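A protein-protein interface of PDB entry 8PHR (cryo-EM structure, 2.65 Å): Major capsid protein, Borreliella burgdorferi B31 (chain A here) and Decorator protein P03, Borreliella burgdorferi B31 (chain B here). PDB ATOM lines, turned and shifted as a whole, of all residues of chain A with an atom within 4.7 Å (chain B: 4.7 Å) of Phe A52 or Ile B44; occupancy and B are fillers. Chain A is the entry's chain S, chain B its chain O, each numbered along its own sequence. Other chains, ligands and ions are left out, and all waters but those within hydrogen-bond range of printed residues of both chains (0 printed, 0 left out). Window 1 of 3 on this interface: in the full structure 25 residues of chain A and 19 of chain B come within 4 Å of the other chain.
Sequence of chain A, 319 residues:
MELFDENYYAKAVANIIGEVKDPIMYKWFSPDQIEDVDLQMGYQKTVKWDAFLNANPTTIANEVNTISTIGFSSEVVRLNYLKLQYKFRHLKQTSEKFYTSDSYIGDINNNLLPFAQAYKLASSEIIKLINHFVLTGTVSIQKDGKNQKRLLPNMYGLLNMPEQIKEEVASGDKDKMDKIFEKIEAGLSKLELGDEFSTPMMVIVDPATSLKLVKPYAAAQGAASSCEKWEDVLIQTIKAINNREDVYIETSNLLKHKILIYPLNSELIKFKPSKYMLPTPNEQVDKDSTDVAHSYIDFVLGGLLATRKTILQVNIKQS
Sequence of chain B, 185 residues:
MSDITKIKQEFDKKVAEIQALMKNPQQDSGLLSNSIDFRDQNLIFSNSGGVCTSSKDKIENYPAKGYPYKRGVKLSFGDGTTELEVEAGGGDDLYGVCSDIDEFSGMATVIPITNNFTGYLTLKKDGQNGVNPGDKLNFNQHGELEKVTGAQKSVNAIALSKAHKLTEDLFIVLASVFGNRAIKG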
ATOM      1  N   ASP A  50      21.330  27.296   6.862  1.00  0.00           N
ATOM      2  CA  ASP A  50      20.251  26.343   6.652  1.00  0.00           C
ATOM      3  C   ASP A  50      20.691  25.268   5.669  1.00  0.00           C
ATOM      4  O   ASP A  50      21.556  25.498   4.819  1.00  0.00           O
ATOM      5  CB  ASP A  50      18.980  27.028   6.125  1.00  0.00           C
ATOM      6  CG  ASP A  50      18.252  27.818   7.195  1.00  0.00           C
ATOM      7  OD1 ASP A  50      18.708  27.815   8.357  1.00  0.00           O
ATOM      8  OD2 ASP A  50      17.220  28.440   6.871  1.00  0.00           O
ATOM      9  N   ALA A  51      20.079  24.092   5.790  1.00  0.00           N
ATOM     10  CA  ALA A  51      20.347  22.967   4.907  1.00  0.00           C
ATOM     11  C   ALA A  51      19.038  22.454   4.327  1.00  0.00           C
ATOM     12  O   ALA A  51      17.978  22.568   4.948  1.00  0.00           O
ATOM     13  CB  ALA A  51      21.070  21.831   5.638  1.00  0.00           C
ATOM     14  N   PHE A  52      19.119  21.885   3.125  1.00  0.00           N
ATOM     15  CA  PHE A  52      17.934  21.387   2.446  1.00  0.00           C
ATOM     16  C   PHE A  52      18.310  20.208   1.562  1.00  0.00           C
ATOM     17  O   PHE A  52      19.472  20.028   1.189  1.00  0.00           O
ATOM     18  CB  PHE A  52      17.255  22.487   1.619  1.00  0.00           C
ATOM     19  CG  PHE A  52      18.188  23.218   0.694  1.00  0.00           C
ATOM     20  CD1 PHE A  52      18.427  22.746  -0.587  1.00  0.00           C
ATOM     21  CD2 PHE A  52      18.824  24.378   1.104  1.00  0.00           C
ATOM     22  CE1 PHE A  52      19.281  23.418  -1.441  1.00  0.00           C
ATOM     23  CE2 PHE A  52      19.681  25.054   0.255  1.00  0.00           C
ATOM     24  CZ  PHE A  52      19.910  24.572  -1.019  1.00  0.00           C
ATOM     25  N   LEU A  53      17.304  19.405   1.229  1.00  0.00           N
ATOM     26  CA  LEU A  53      17.470  18.245   0.363  1.00  0.00           C
ATOM     27  C   LEU A  53      17.060  18.614  -1.055  1.00  0.00           C
ATOM     28  O   LEU A  53      15.983  19.182  -1.268  1.00  0.00           O
ATOM     29  CB  LEU A  53      16.639  17.063   0.866  1.00  0.00           C
ATOM     30  CG  LEU A  53      16.801  16.680   2.339  1.00  0.00           C
ATOM     31  CD1 LEU A  53      16.033  15.404   2.650  1.00  0.00           C
ATOM     32  CD2 LEU A  53      18.270  16.523   2.698  1.00  0.00           C
ATOM     33  N   ASN A  54      17.917  18.290  -2.022  1.00  0.00           N
ATOM     34  CA  ASN A  54      17.671  18.657  -3.411  1.00  0.00           C
ATOM     35  C   ASN A  54      16.798  17.652  -4.148  1.00  0.00           C
ATOM     36  O   ASN A  54      16.020  18.047  -5.024  1.00  0.00           O
ATOM     37  CB  ASN A  54      18.999  18.814  -4.158  1.00  0.00           C
ATOM     38  CG  ASN A  54      19.724  20.093  -3.792  1.00  0.00           C
ATOM     39  OD1 ASN A  54      19.252  21.193  -4.084  1.00  0.00           O
ATOM     40  ND2 ASN A  54      20.878  19.957  -3.150  1.00  0.00           N
ATOM     41  N   ILE A  70      22.843  17.405  -1.128  1.00  0.00           N
ATOM     42  CA  ILE A  70      22.229  18.176  -0.054  1.00  0.00           C
ATOM     43  C   ILE A  70      22.796  19.586  -0.122  1.00  0.00           C
ATOM     44  O   ILE A  70      24.017  19.776  -0.033  1.00  0.00           O
ATOM     45  CB  ILE A  70      22.485  17.542   1.322  1.00  0.00           C
ATOM     46  CG1 ILE A  70      21.748  16.208   1.447  1.00  0.00           C
ATOM     47  CG2 ILE A  70      22.073  18.495   2.436  1.00  0.00           C
ATOM     48  CD1 ILE A  70      21.969  15.516   2.773  1.00  0.00           C
ATOM     49  N   GLY A  71      21.916  20.573  -0.277  1.00  0.00           N
ATOM     50  CA  GLY A  71      22.333  21.945  -0.449  1.00  0.00           C
ATOM     51  C   GLY A  71      22.324  22.727   0.850  1.00  0.00           C
ATOM     52  O   GLY A  71      21.667  22.358   1.822  1.00  0.00           O
ATOM     53  N   PHE A  72      23.063  23.833   0.847  1.00  0.00           N
ATOM     54  CA  PHE A  72      23.181  24.709   2.001  1.00  0.00           C
ATOM     55  C   PHE A  72      22.937  26.147   1.570  1.00  0.00           C
ATOM     56  O   PHE A  72      23.098  26.504   0.400  1.00  0.00           O
ATOM     57  CB  PHE A  72      24.558  24.584   2.664  1.00  0.00           C
ATOM     58  CG  PHE A  72      24.898  23.188   3.101  1.00  0.00           C
ATOM     59  CD1 PHE A  72      24.243  22.605   4.173  1.00  0.00           C
ATOM     60  CD2 PHE A  72      25.873  22.459   2.442  1.00  0.00           C
ATOM     61  CE1 PHE A  72      24.554  21.320   4.579  1.00  0.00           C
ATOM     62  CE2 PHE A  72      26.189  21.174   2.842  1.00  0.00           C
ATOM     63  CZ  PHE A  72      25.528  20.604   3.912  1.00  0.00           C
ATOM     64  N   SER A  73      22.544  26.976   2.535  1.00  0.00           N
ATOM     65  CA  SER A  73      22.232  28.370   2.257  1.00  0.00           C
ATOM     66  C   SER A  73      22.568  29.220   3.472  1.00  0.00           C
ATOM     67  O   SER A  73      22.419  28.776   4.614  1.00  0.00           O
ATOM     68  CB  SER A  73      20.756  28.548   1.881  1.00  0.00           C
ATOM     69  OG  SER A  73      19.908  28.153   2.944  1.00  0.00           O
ATOM     70  N   GLN B  41      12.112  22.979   0.422  1.00  0.00           N
ATOM     71  CA  GLN B  41      13.037  23.996   0.908  1.00  0.00           C
ATOM     72  C   GLN B  41      14.226  24.192  -0.027  1.00  0.00           C
ATOM     73  O   GLN B  41      15.260  24.721   0.394  1.00  0.00           O
ATOM     74  CB  GLN B  41      13.522  23.644   2.315  1.00  0.00           C
ATOM     75  CG  GLN B  41      12.480  23.842   3.401  1.00  0.00           C
ATOM     76  CD  GLN B  41      13.068  23.727   4.793  1.00  0.00           C
ATOM     77  OE1 GLN B  41      14.249  23.420   4.958  1.00  0.00           O
ATOM     78  NE2 GLN B  41      12.243  23.974   5.805  1.00  0.00           N
ATOM     79  N   ASN B  42      14.099  23.785  -1.289  1.00  0.00           N
ATOM     80  CA  ASN B  42      15.187  23.891  -2.250  1.00  0.00           C
ATOM     81  C   ASN B  42      14.852  24.761  -3.453  1.00  0.00           C
ATOM     82  O   ASN B  42      15.696  24.906  -4.345  1.00  0.00           O
ATOM     83  CB  ASN B  42      15.608  22.496  -2.734  1.00  0.00           C
ATOM     84  CG  ASN B  42      14.522  21.804  -3.533  1.00  0.00           C
ATOM     85  OD1 ASN B  42      13.401  21.629  -3.055  1.00  0.00           O
ATOM     86  ND2 ASN B  42      14.849  21.409  -4.757  1.00  0.00           N
ATOM     87  N   LEU B  43      13.654  25.342  -3.507  1.00  0.00           N
ATOM     88  CA  LEU B  43      13.256  26.191  -4.629  1.00  0.00           C
ATOM     89  C   LEU B  43      13.715  27.627  -4.370  1.00  0.00           C
ATOM     90  O   LEU B  43      12.927  28.547  -4.144  1.00  0.00           O
ATOM     91  CB  LEU B  43      11.751  26.112  -4.850  1.00  0.00           C
ATOM     92  CG  LEU B  43      11.192  24.733  -5.208  1.00  0.00           C
ATOM     93  CD1 LEU B  43       9.754  24.845  -5.687  1.00  0.00           C
ATOM     94  CD2 LEU B  43      12.059  24.054  -6.258  1.00  0.00           C
ATOM     95  N   ILE B  44      15.034  27.803  -4.407  1.00  0.00           N
ATOM     96  CA  ILE B  44      15.664  29.098  -4.185  1.00  0.00           C
ATOM     97  C   ILE B  44      16.673  29.353  -5.294  1.00  0.00           C
ATOM     98  O   ILE B  44      17.195  28.420  -5.913  1.00  0.00           O
ATOM     99  CB  ILE B  44      16.343  29.177  -2.798  1.00  0.00           C
ATOM    100  CG1 ILE B  44      17.376  28.059  -2.644  1.00  0.00           C
ATOM    101  CG2 ILE B  44      15.307  29.118  -1.687  1.00  0.00           C
ATOM    102  CD1 ILE B  44      18.166  28.130  -1.356  1.00  0.00           C
ATOM    103  N   PHE B  45      16.947  30.635  -5.544  1.00  0.00           N
ATOM    104  CA  PHE B  45      17.889  31.009  -6.592  1.00  0.00           C
ATOM    105  C   PHE B  45      19.335  30.734  -6.202  1.00  0.00           C
ATOM    106  O   PHE B  45      20.186  30.598  -7.088  1.00  0.00           O
ATOM    107  CB  PHE B  45      17.722  32.486  -6.951  1.00  0.00           C
ATOM    108  CG  PHE B  45      18.089  32.808  -8.371  1.00  0.00           C
ATOM    109  CD1 PHE B  45      17.448  32.178  -9.425  1.00  0.00           C
ATOM    110  CD2 PHE B  45      19.075  33.738  -8.651  1.00  0.00           C
ATOM    111  CE1 PHE B  45      17.784  32.472 -10.734  1.00  0.00           C
ATOM    112  CE2 PHE B  45      19.416  34.037  -9.957  1.00  0.00           C
ATOM    113  CZ  PHE B  45      18.769  33.403 -10.999  1.00  0.00           C
ATOM    114  N   SER B  46      19.633  30.651  -4.908  1.00  0.00           N
ATOM    115  CA  SER B  46      20.991  30.404  -4.442  1.00  0.00           C
ATOM    116  C   SER B  46      21.352  28.923  -4.420  1.00  0.00           C
ATOM    117  O   SER B  46      22.409  28.567  -3.891  1.00  0.00           O
ATOM    118  CB  SER B  46      21.187  31.007  -3.048  1.00  0.00           C
ATOM    119  OG  SER B  46      20.210  30.525  -2.142  1.00  0.00           O
ATOM    120  N   ASN B  47      20.505  28.060  -4.981  1.00  0.00           N
ATOM    121  CA  ASN B  47      20.778  26.624  -5.041  1.00  0.00           C
ATOM    122  C   ASN B  47      21.699  26.362  -6.229  1.00  0.00           C
ATOM    123  O   ASN B  47      21.280  25.950  -7.313  1.00  0.00           O
ATOM    124  CB  ASN B  47      19.481  25.832  -5.145  1.00  0.00           C
ATOM    125  CG  ASN B  47      19.677  24.353  -4.874  1.00  0.00           C
ATOM    126  OD1 ASN B  47      20.775  23.914  -4.531  1.00  0.00           O
ATOM    127  ND2 ASN B  47      18.611  23.577  -5.027  1.00  0.00           N
ATOM    128  N   LEU B 166       9.875  32.449  -8.658  1.00  0.00           N
ATOM    129  CA  LEU B 166      10.598  33.071  -7.555  1.00  0.00           C
ATOM    130  C   LEU B 166      10.330  34.565  -7.462  1.00  0.00           C
ATOM    131  O   LEU B 166      10.332  35.122  -6.358  1.00  0.00           O
ATOM    132  CB  LEU B 166      12.104  32.833  -7.706  1.00  0.00           C
ATOM    133  CG  LEU B 166      12.583  31.380  -7.690  1.00  0.00           C
ATOM    134  CD1 LEU B 166      14.090  31.321  -7.494  1.00  0.00           C
ATOM    135  CD2 LEU B 166      11.867  30.585  -6.608  1.00  0.00           C
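The backbone NH (N) of Phe A52 is in hydrogen-bond range of the backbone carbonyl oxygen (O) of Gly A71 (2.9 Å).
The side-chain amide nitrogen (ND2) of Asn A54 lies close to the backbone NH (N) of Gly A71, at 3.1 Å.
O of Asn B42 is in hydrogen-bond range of ND2 of Asn B47 (3.3 Å).
The side-chain amide oxygen of Asn A54 is in hydrogen-bond range of the side-chain amide nitrogen of Asn B47, 2.6 Å away.
Printed residues of chain A that touch a printed residue of chain B: Ala A51, Phe A52, Leu A53 and Asn A54.
Hydrophobic or aromatic side chains of chain A within 4 Å of the printed part of chain B: Phe A52.
Along chain A the printed residues that touch a printed residue of chain B span positions 51 to 54.
Along chain B the printed residues that touch a printed residue of chain A span positions 41 to 47.
Among the printed residues, 8 pairs touch across the chains.
Gln B41 touches Ala A51.
CB of Phe A52 touches O of Gln B41, at 3.2 Å.
Phe A52 touches Asn B42 (CD1 to CB, 3.6 Å).
Phe A52 touches Ile B44.
CE1 of Phe A52 touches OD1 of Asn B47 (3.5 Å).
Leu A53 touches Asn B42.
Asn A54 touches Asn B42.
Of the printed residues of chain B, Ala A51 touches Gln B41 (3.8 Å).
Of the printed residues of chain B, Asn A54 touches Asn B42 and Asn B47.
Of the printed residues of chain A, Asn B42 touches Phe A52 (3.6 Å), Leu A53 (3.6 Å) and Asn A54 (3.6 Å).
Ile B44 touches just one residue of chain A: Phe A52.
Of the printed residues of chain A, Asn B47 touches Phe A52 and Asn A54.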
